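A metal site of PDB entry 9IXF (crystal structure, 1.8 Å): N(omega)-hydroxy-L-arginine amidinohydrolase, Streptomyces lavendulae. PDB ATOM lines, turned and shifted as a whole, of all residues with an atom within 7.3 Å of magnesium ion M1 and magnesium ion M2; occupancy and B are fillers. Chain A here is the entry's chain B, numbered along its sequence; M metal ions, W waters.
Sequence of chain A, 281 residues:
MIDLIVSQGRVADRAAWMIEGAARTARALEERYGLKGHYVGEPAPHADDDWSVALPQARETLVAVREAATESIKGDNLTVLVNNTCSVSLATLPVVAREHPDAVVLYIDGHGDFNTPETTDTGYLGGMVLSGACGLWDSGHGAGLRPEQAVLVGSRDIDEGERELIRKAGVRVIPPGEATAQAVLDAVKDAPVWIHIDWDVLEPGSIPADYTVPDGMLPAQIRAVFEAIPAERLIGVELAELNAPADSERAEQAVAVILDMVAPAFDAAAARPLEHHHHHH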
ATOM      1  N   MET A  18      -3.240  12.081   7.157  1.00  0.00           N
ATOM      2  CA  MET A  18      -4.465  12.859   7.316  1.00  0.00           C
ATOM      3  C   MET A  18      -4.545  13.542   8.681  1.00  0.00           C
ATOM      4  O   MET A  18      -5.184  14.600   8.805  1.00  0.00           O
ATOM      5  CB  MET A  18      -5.690  11.967   7.034  1.00  0.00           C
ATOM      6  CG  MET A  18      -6.017  11.914   5.510  1.00  0.00           C
ATOM      7  SD  MET A  18      -7.294  10.728   5.083  1.00  0.00           S
ATOM      8  CE  MET A  18      -6.693   9.380   6.050  1.00  0.00           C
ATOM      9  N   THR A  85     -10.460  12.659   9.108  1.00  0.00           N
ATOM     10  CA  THR A  85     -11.244  11.839   8.184  1.00  0.00           C
ATOM     11  C   THR A  85     -12.708  12.248   8.208  1.00  0.00           C
ATOM     12  O   THR A  85     -13.181  12.818   9.188  1.00  0.00           O
ATOM     13  CB  THR A  85     -11.150  10.349   8.534  1.00  0.00           C
ATOM     14  OG1 THR A  85     -11.773  10.117   9.803  1.00  0.00           O
ATOM     15  CG2 THR A  85      -9.707   9.884   8.588  1.00  0.00           C
ATOM     16  N   CYS A  86     -13.417  11.911   7.127  1.00  0.00           N
ATOM     17  CA  CYS A  86     -14.874  12.089   7.092  1.00  0.00           C
ATOM     18  C   CYS A  86     -15.561  11.343   8.226  1.00  0.00           C
ATOM     19  O   CYS A  86     -16.632  11.749   8.668  1.00  0.00           O
ATOM     20  CB  CYS A  86     -15.441  11.590   5.766  1.00  0.00           C
ATOM     21  SG  CYS A  86     -15.337  12.744   4.389  1.00  0.00           S
ATOM     22  N   SER A  87     -14.973  10.236   8.698  1.00  0.00           N
ATOM     23  CA  SER A  87     -15.630   9.415   9.719  1.00  0.00           C
ATOM     24  C   SER A  87     -15.833  10.160  11.024  1.00  0.00           C
ATOM     25  O   SER A  87     -16.671   9.760  11.821  1.00  0.00           O
ATOM     26  CB  SER A  87     -14.838   8.142   9.989  1.00  0.00           C
ATOM     27  OG  SER A  87     -14.737   7.364   8.817  1.00  0.00           O
ATOM     28  N   TYR A 107     -23.241  17.999   1.831  1.00  0.00           N
ATOM     29  CA  TYR A 107     -22.197  16.992   1.974  1.00  0.00           C
ATOM     30  C   TYR A 107     -21.409  17.042   0.674  1.00  0.00           C
ATOM     31  O   TYR A 107     -21.783  16.443  -0.321  1.00  0.00           O
ATOM     32  CB  TYR A 107     -22.796  15.606   2.241  1.00  0.00           C
ATOM     33  CG  TYR A 107     -21.811  14.634   2.842  1.00  0.00           C
ATOM     34  CD1 TYR A 107     -20.956  13.892   2.026  1.00  0.00           C
ATOM     35  CD2 TYR A 107     -21.740  14.453   4.214  1.00  0.00           C
ATOM     36  CE1 TYR A 107     -20.048  13.002   2.563  1.00  0.00           C
ATOM     37  CE2 TYR A 107     -20.824  13.550   4.775  1.00  0.00           C
ATOM     38  CZ  TYR A 107     -19.982  12.833   3.942  1.00  0.00           C
ATOM     39  OH  TYR A 107     -19.078  11.951   4.476  1.00  0.00           O
ATOM     40  N   ILE A 108     -20.340  17.837   0.681  1.00  0.00           N
ATOM     41  CA  ILE A 108     -19.591  18.120  -0.540  1.00  0.00           C
ATOM     42  C   ILE A 108     -18.454  17.112  -0.635  1.00  0.00           C
ATOM     43  O   ILE A 108     -17.501  17.159   0.145  1.00  0.00           O
ATOM     44  CB  ILE A 108     -19.073  19.563  -0.552  1.00  0.00           C
ATOM     45  CG1 ILE A 108     -20.236  20.534  -0.260  1.00  0.00           C
ATOM     46  CG2 ILE A 108     -18.438  19.841  -1.918  1.00  0.00           C
ATOM     47  CD1 ILE A 108     -19.868  22.033  -0.310  1.00  0.00           C
ATOM     48  N   ASP A 109     -18.562  16.175  -1.575  1.00  0.00           N
ATOM     49  CA  ASP A 109     -17.793  14.946  -1.514  1.00  0.00           C
ATOM     50  C   ASP A 109     -17.742  14.321  -2.907  1.00  0.00           C
ATOM     51  O   ASP A 109     -18.738  14.359  -3.638  1.00  0.00           O
ATOM     52  CB  ASP A 109     -18.469  13.989  -0.497  1.00  0.00           C
ATOM     53  CG  ASP A 109     -17.604  12.808  -0.107  1.00  0.00           C
ATOM     54  OD1 ASP A 109     -17.609  11.790  -0.858  1.00  0.00           O
ATOM     55  OD2 ASP A 109     -16.975  12.878   0.977  1.00  0.00           O
ATOM     56  N   GLY A 110     -16.602  13.734  -3.256  1.00  0.00           N
ATOM     57  CA  GLY A 110     -16.495  13.085  -4.547  1.00  0.00           C
ATOM     58  C   GLY A 110     -17.222  11.758  -4.662  1.00  0.00           C
ATOM     59  O   GLY A 110     -17.442  11.279  -5.774  1.00  0.00           O
ATOM     60  N   HIS A 111     -17.627  11.166  -3.539  1.00  0.00           N
ATOM     61  CA  HIS A 111     -18.119   9.789  -3.535  1.00  0.00           C
ATOM     62  C   HIS A 111     -19.562   9.614  -3.106  1.00  0.00           C
ATOM     63  O   HIS A 111     -20.279   8.807  -3.701  1.00  0.00           O
ATOM     64  CB  HIS A 111     -17.237   8.933  -2.634  1.00  0.00           C
ATOM     65  CG  HIS A 111     -15.853   8.768  -3.154  1.00  0.00           C
ATOM     66  ND1 HIS A 111     -15.491   7.738  -4.004  1.00  0.00           N
ATOM     67  CD2 HIS A 111     -14.739   9.509  -2.976  1.00  0.00           C
ATOM     68  CE1 HIS A 111     -14.212   7.849  -4.301  1.00  0.00           C
ATOM     69  NE2 HIS A 111     -13.729   8.917  -3.688  1.00  0.00           N
ATOM     70  N   GLY A 112     -20.014  10.302  -2.066  1.00  0.00           N
ATOM     71  CA  GLY A 112     -21.338  10.115  -1.519  1.00  0.00           C
ATOM     72  C   GLY A 112     -21.354   9.512  -0.121  1.00  0.00           C
ATOM     73  O   GLY A 112     -22.244   9.829   0.670  1.00  0.00           O
ATOM     74  N   ASP A 113     -20.384   8.644   0.191  1.00  0.00           N
ATOM     75  CA  ASP A 113     -20.204   8.084   1.536  1.00  0.00           C
ATOM     76  C   ASP A 113     -21.517   7.581   2.120  1.00  0.00           C
ATOM     77  O   ASP A 113     -21.851   7.813   3.290  1.00  0.00           O
ATOM     78  CB  ASP A 113     -19.556   9.114   2.462  1.00  0.00           C
ATOM     79  CG  ASP A 113     -18.181   9.526   1.976  1.00  0.00           C
ATOM     80  OD1 ASP A 113     -17.637   8.821   1.086  1.00  0.00           O
ATOM     81  OD2 ASP A 113     -17.645  10.526   2.505  1.00  0.00           O
ATOM     82  N   TYR A 124     -14.519   0.334   4.295  1.00  0.00           N
ATOM     83  CA  TYR A 124     -14.000   1.616   4.796  1.00  0.00           C
ATOM     84  C   TYR A 124     -15.084   2.419   5.489  1.00  0.00           C
ATOM     85  O   TYR A 124     -16.083   2.815   4.854  1.00  0.00           O
ATOM     86  CB  TYR A 124     -13.418   2.421   3.644  1.00  0.00           C
ATOM     87  CG  TYR A 124     -12.812   3.738   4.084  1.00  0.00           C
ATOM     88  CD1 TYR A 124     -12.014   3.812   5.219  1.00  0.00           C
ATOM     89  CD2 TYR A 124     -13.020   4.901   3.337  1.00  0.00           C
ATOM     90  CE1 TYR A 124     -11.443   5.021   5.617  1.00  0.00           C
ATOM     91  CE2 TYR A 124     -12.448   6.112   3.744  1.00  0.00           C
ATOM     92  CZ  TYR A 124     -11.674   6.160   4.866  1.00  0.00           C
ATOM     93  OH  TYR A 124     -11.115   7.371   5.253  1.00  0.00           O
ATOM     94  N   GLY A 126     -15.054   5.439   6.285  1.00  0.00           N
ATOM     95  CA  GLY A 126     -15.191   6.759   5.692  1.00  0.00           C
ATOM     96  C   GLY A 126     -16.159   6.817   4.539  1.00  0.00           C
ATOM     97  O   GLY A 126     -16.588   7.909   4.155  1.00  0.00           O
ATOM     98  N   GLY A 127     -16.524   5.668   3.970  1.00  0.00           N
ATOM     99  CA  GLY A 127     -17.538   5.590   2.939  1.00  0.00           C
ATOM    100  C   GLY A 127     -18.921   5.252   3.456  1.00  0.00           C
ATOM    101  O   GLY A 127     -19.814   4.984   2.645  1.00  0.00           O
ATOM    102  N   VAL A 129     -20.396   7.306   6.100  1.00  0.00           N
ATOM    103  CA  VAL A 129     -20.637   8.389   7.050  1.00  0.00           C
ATOM    104  C   VAL A 129     -22.038   8.980   6.888  1.00  0.00           C
ATOM    105  O   VAL A 129     -22.771   9.140   7.869  1.00  0.00           O
ATOM    106  CB  VAL A 129     -19.569   9.487   6.878  1.00  0.00           C
ATOM    107  CG1 VAL A 129     -19.900  10.689   7.793  1.00  0.00           C
ATOM    108  CG2 VAL A 129     -18.205   8.921   7.189  1.00  0.00           C
ATOM    109  N   HIS A 196     -20.201  20.229   4.982  1.00  0.00           N
ATOM    110  CA  HIS A 196     -19.195  19.196   5.175  1.00  0.00           C
ATOM    111  C   HIS A 196     -18.430  19.076   3.881  1.00  0.00           C
ATOM    112  O   HIS A 196     -19.033  18.833   2.835  1.00  0.00           O
ATOM    113  CB  HIS A 196     -19.887  17.872   5.537  1.00  0.00           C
ATOM    114  CG  HIS A 196     -18.955  16.696   5.594  1.00  0.00           C
ATOM    115  ND1 HIS A 196     -18.591  16.097   6.773  1.00  0.00           N
ATOM    116  CD2 HIS A 196     -18.366  15.985   4.602  1.00  0.00           C
ATOM    117  CE1 HIS A 196     -17.780  15.085   6.523  1.00  0.00           C
ATOM    118  NE2 HIS A 196     -17.623  14.990   5.209  1.00  0.00           N
ATOM    119  N   ILE A 197     -17.108  19.275   3.902  1.00  0.00           N
ATOM    120  CA  ILE A 197     -16.368  19.121   2.649  1.00  0.00           C
ATOM    121  C   ILE A 197     -15.203  18.139   2.797  1.00  0.00           C
ATOM    122  O   ILE A 197     -14.388  18.243   3.726  1.00  0.00           O
ATOM    123  CB  ILE A 197     -15.900  20.473   2.080  1.00  0.00           C
ATOM    124  CG1 ILE A 197     -15.293  20.282   0.681  1.00  0.00           C
ATOM    125  CG2 ILE A 197     -14.963  21.177   3.027  1.00  0.00           C
ATOM    126  CD1 ILE A 197     -15.397  21.573  -0.195  1.00  0.00           C
ATOM    127  N   ASP A 198     -15.165  17.153   1.881  1.00  0.00           N
ATOM    128  CA  ASP A 198     -14.079  16.204   1.676  1.00  0.00           C
ATOM    129  C   ASP A 198     -13.319  16.655   0.428  1.00  0.00           C
ATOM    130  O   ASP A 198     -13.911  16.728  -0.655  1.00  0.00           O
ATOM    131  CB  ASP A 198     -14.682  14.804   1.499  1.00  0.00           C
ATOM    132  CG  ASP A 198     -13.664  13.681   1.281  1.00  0.00           C
ATOM    133  OD1 ASP A 198     -12.502  13.908   0.899  1.00  0.00           O
ATOM    134  OD2 ASP A 198     -14.077  12.504   1.489  1.00  0.00           O
ATOM    135  N   TRP A 199     -12.026  16.979   0.570  1.00  0.00           N
ATOM    136  CA  TRP A 199     -11.291  17.515  -0.578  1.00  0.00           C
ATOM    137  C   TRP A 199     -11.208  16.572  -1.776  1.00  0.00           C
ATOM    138  O   TRP A 199     -10.807  17.036  -2.862  1.00  0.00           O
ATOM    139  CB  TRP A 199      -9.877  17.942  -0.153  1.00  0.00           C
ATOM    140  CG  TRP A 199      -9.945  18.928   0.970  1.00  0.00           C
ATOM    141  CD1 TRP A 199      -9.401  18.788   2.218  1.00  0.00           C
ATOM    142  CD2 TRP A 199     -10.638  20.178   0.977  1.00  0.00           C
ATOM    143  NE1 TRP A 199      -9.711  19.881   2.998  1.00  0.00           N
ATOM    144  CE2 TRP A 199     -10.470  20.750   2.260  1.00  0.00           C
ATOM    145  CE3 TRP A 199     -11.394  20.882   0.016  1.00  0.00           C
ATOM    146  CZ2 TRP A 199     -11.003  21.979   2.606  1.00  0.00           C
ATOM    147  CZ3 TRP A 199     -11.936  22.110   0.372  1.00  0.00           C
ATOM    148  CH2 TRP A 199     -11.748  22.635   1.658  1.00  0.00           C
ATOM    149  N   ASP A 200     -11.587  15.298  -1.644  1.00  0.00           N
ATOM    150  CA  ASP A 200     -11.634  14.475  -2.845  1.00  0.00           C
ATOM    151  C   ASP A 200     -12.730  14.925  -3.809  1.00  0.00           C
ATOM    152  O   ASP A 200     -12.782  14.406  -4.940  1.00  0.00           O
ATOM    153  CB  ASP A 200     -11.755  12.975  -2.493  1.00  0.00           C
ATOM    154  CG  ASP A 200     -13.079  12.577  -1.803  1.00  0.00           C
ATOM    155  OD1 ASP A 200     -14.134  13.168  -2.099  1.00  0.00           O
ATOM    156  OD2 ASP A 200     -13.072  11.615  -0.979  1.00  0.00           O
ATOM    157  N   VAL A 201     -13.591  15.862  -3.422  1.00  0.00           N
ATOM    158  CA  VAL A 201     -14.572  16.411  -4.351  1.00  0.00           C
ATOM    159  C   VAL A 201     -13.898  17.159  -5.496  1.00  0.00           C
ATOM    160  O   VAL A 201     -14.471  17.259  -6.597  1.00  0.00           O
ATOM    161  CB  VAL A 201     -15.577  17.321  -3.615  1.00  0.00           C
ATOM    162  CG1 VAL A 201     -14.913  18.623  -3.202  1.00  0.00           C
ATOM    163  CG2 VAL A 201     -16.787  17.602  -4.499  1.00  0.00           C
ATOM    164  N   ALA A 209      -5.280  14.096  -1.696  1.00  0.00           N
ATOM    165  CA  ALA A 209      -6.246  13.332  -0.922  1.00  0.00           C
ATOM    166  C   ALA A 209      -6.241  11.905  -1.442  1.00  0.00           C
ATOM    167  O   ALA A 209      -5.836  11.646  -2.583  1.00  0.00           O
ATOM    168  CB  ALA A 209      -7.652  13.951  -1.019  1.00  0.00           C
ATOM    169  N   ASP A 210      -6.672  10.970  -0.596  1.00  0.00           N
ATOM    170  CA  ASP A 210      -6.844   9.611  -1.064  1.00  0.00           C
ATOM    171  C   ASP A 210      -8.219   9.458  -1.712  1.00  0.00           C
ATOM    172  O   ASP A 210      -9.112  10.288  -1.524  1.00  0.00           O
ATOM    173  CB  ASP A 210      -6.659   8.609   0.084  1.00  0.00           C
ATOM    174  CG  ASP A 210      -7.697   8.776   1.197  1.00  0.00           C
ATOM    175  OD1 ASP A 210      -8.280   9.882   1.318  1.00  0.00           O
ATOM    176  OD2 ASP A 210      -7.922   7.801   1.961  1.00  0.00           O
ATOM    177  N   TYR A 211      -8.378   8.402  -2.504  1.00  0.00           N
ATOM    178  CA  TYR A 211      -9.630   8.131  -3.211  1.00  0.00           C
ATOM    179  C   TYR A 211     -10.002   9.260  -4.167  1.00  0.00           C
ATOM    180  O   TYR A 211     -11.155   9.686  -4.240  1.00  0.00           O
ATOM    181  CB  TYR A 211     -10.775   7.882  -2.219  1.00  0.00           C
ATOM    182  CG  TYR A 211     -10.610   6.685  -1.318  1.00  0.00           C
ATOM    183  CD1 TYR A 211     -10.839   5.399  -1.796  1.00  0.00           C
ATOM    184  CD2 TYR A 211     -10.256   6.822   0.016  1.00  0.00           C
ATOM    185  CE1 TYR A 211     -10.702   4.290  -0.982  1.00  0.00           C
ATOM    186  CE2 TYR A 211     -10.110   5.723   0.849  1.00  0.00           C
ATOM    187  CZ  TYR A 211     -10.342   4.462   0.343  1.00  0.00           C
ATOM    188  OH  TYR A 211     -10.214   3.346   1.148  1.00  0.00           O
ATOM    189  N   THR A 212      -9.009   9.771  -4.911  1.00  0.00           N
ATOM    190  CA  THR A 212      -9.290  10.772  -5.944  1.00  0.00           C
ATOM    191  C   THR A 212     -10.177  10.168  -7.024  1.00  0.00           C
ATOM    192  O   THR A 212     -10.170   8.944  -7.238  1.00  0.00           O
ATOM    193  CB  THR A 212      -7.980  11.299  -6.557  1.00  0.00           C
ATOM    194  OG1 THR A 212      -7.360  10.275  -7.335  1.00  0.00           O
ATOM    195  CG2 THR A 212      -7.022  11.744  -5.474  1.00  0.00           C
ATOM    196  N   ALA A 240     -12.260  18.282   5.729  1.00  0.00           N
ATOM    197  CA  ALA A 240     -11.693  16.971   5.999  1.00  0.00           C
ATOM    198  C   ALA A 240     -10.868  16.428   4.846  1.00  0.00           C
ATOM    199  O   ALA A 240     -11.172  16.670   3.675  1.00  0.00           O
ATOM    200  CB  ALA A 240     -12.800  15.952   6.315  1.00  0.00           C
ATOM    201  N   GLU A 241      -9.819  15.670   5.211  1.00  0.00           N
ATOM    202  CA  GLU A 241      -9.130  14.657   4.399  1.00  0.00           C
ATOM    203  C   GLU A 241      -8.031  15.211   3.507  1.00  0.00           C
ATOM    204  O   GLU A 241      -7.754  14.660   2.438  1.00  0.00           O
ATOM    205  CB  GLU A 241     -10.139  13.847   3.564  1.00  0.00           C
ATOM    206  CG  GLU A 241     -11.175  13.176   4.458  1.00  0.00           C
ATOM    207  CD  GLU A 241     -11.572  11.808   4.013  1.00  0.00           C
ATOM    208  OE1 GLU A 241     -12.003  11.030   4.887  1.00  0.00           O
ATOM    209  OE2 GLU A 241     -11.464  11.502   2.801  1.00  0.00           O
HETATM  210 MG    MG M   1     -15.861  11.536   2.110  1.00  0.00          MG
HETATM  211 MG    MG M   2     -12.192  11.610   0.907  1.00  0.00          MG
HETATM  212  O   HOH W   1     -12.589   9.668   1.093  1.00  0.00           O
HETATM  213  O   HOH W   2     -10.192  11.505   0.331  1.00  0.00           O
HETATM  214  O   HOH W   3     -15.452  10.488   0.320  1.00  0.00           O
HETATM  215  O   HOH W   4     -14.859  10.002   3.079  1.00  0.00           O
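OE1 of Glu 241 is in hydrogen-bond range of N of Cys 86 (2.8 Å).
The backbone NH (N) of His 111 is in hydrogen-bond range of the side-chain carboxylate (OD1) of Asp 109.
OD1 of Asp 109 is in hydrogen-bond range of N of Gly 112 (3.1 Å).
The backbone NH of Gly 110 is in hydrogen-bond range of the side-chain carboxylate of Asp 200 (2.8 Å).
The side-chain hydroxyl (OH) of Tyr 107 sits close to the side-chain carboxylate (OD2) of Asp 113, at 2.8 Å.
The backbone NH (N) of Val 129 lies within hydrogen-bond range of the backbone carbonyl oxygen (O) of Asp 113 (3.2 Å).
The backbone NH of Asp 198 is in hydrogen-bond range of the backbone carbonyl oxygen of Ile 108, at 2.9 Å.
SG of Cys 86 lies close to NE2 of His 196, at 3.3 Å.
The nearest printed residue that does not touch magnesium ion M1 is Tyr 107 (4.01 Å).
Water W4 binds magnesium ion M1 (2.1 Å).
OD2 of Asp 109 binds magnesium ion M1, at 2.1 Å.
The side-chain carboxylate (OD2) of Asp 113 is bound to magnesium ion M1 (2.1 Å).
Water W3 binds magnesium ion M1, at 2.1 Å.
The side-chain carboxylate (OD2) of Asp 198 binds magnesium ion M1 (2.1 Å).
The side-chain sulfur (SG) of Cys 86 is bound to magnesium ion M1, at 2.6 Å.
Magnesium ion M1 has six donor atoms within binding distance.
Magnesium ion M2 is bound by water W1 (2.0 Å), the side-chain carboxylate (OE2) of Glu 241 (2.0 Å), the side-chain carboxylate (OD2) of Asp 200 (2.1 Å), water W2 (2.1 Å), the side-chain carboxylate (OD2) of Asp 198 (2.2 Å) and the side-chain carboxylate (OD1) of Asp 198 (2.3 Å).
Water W3 bridges the side-chain carboxylate (OD1) of Asp 109 (2.8 Å) and the side-chain carboxylate (OD1) of Asp 113 (2.9 Å).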
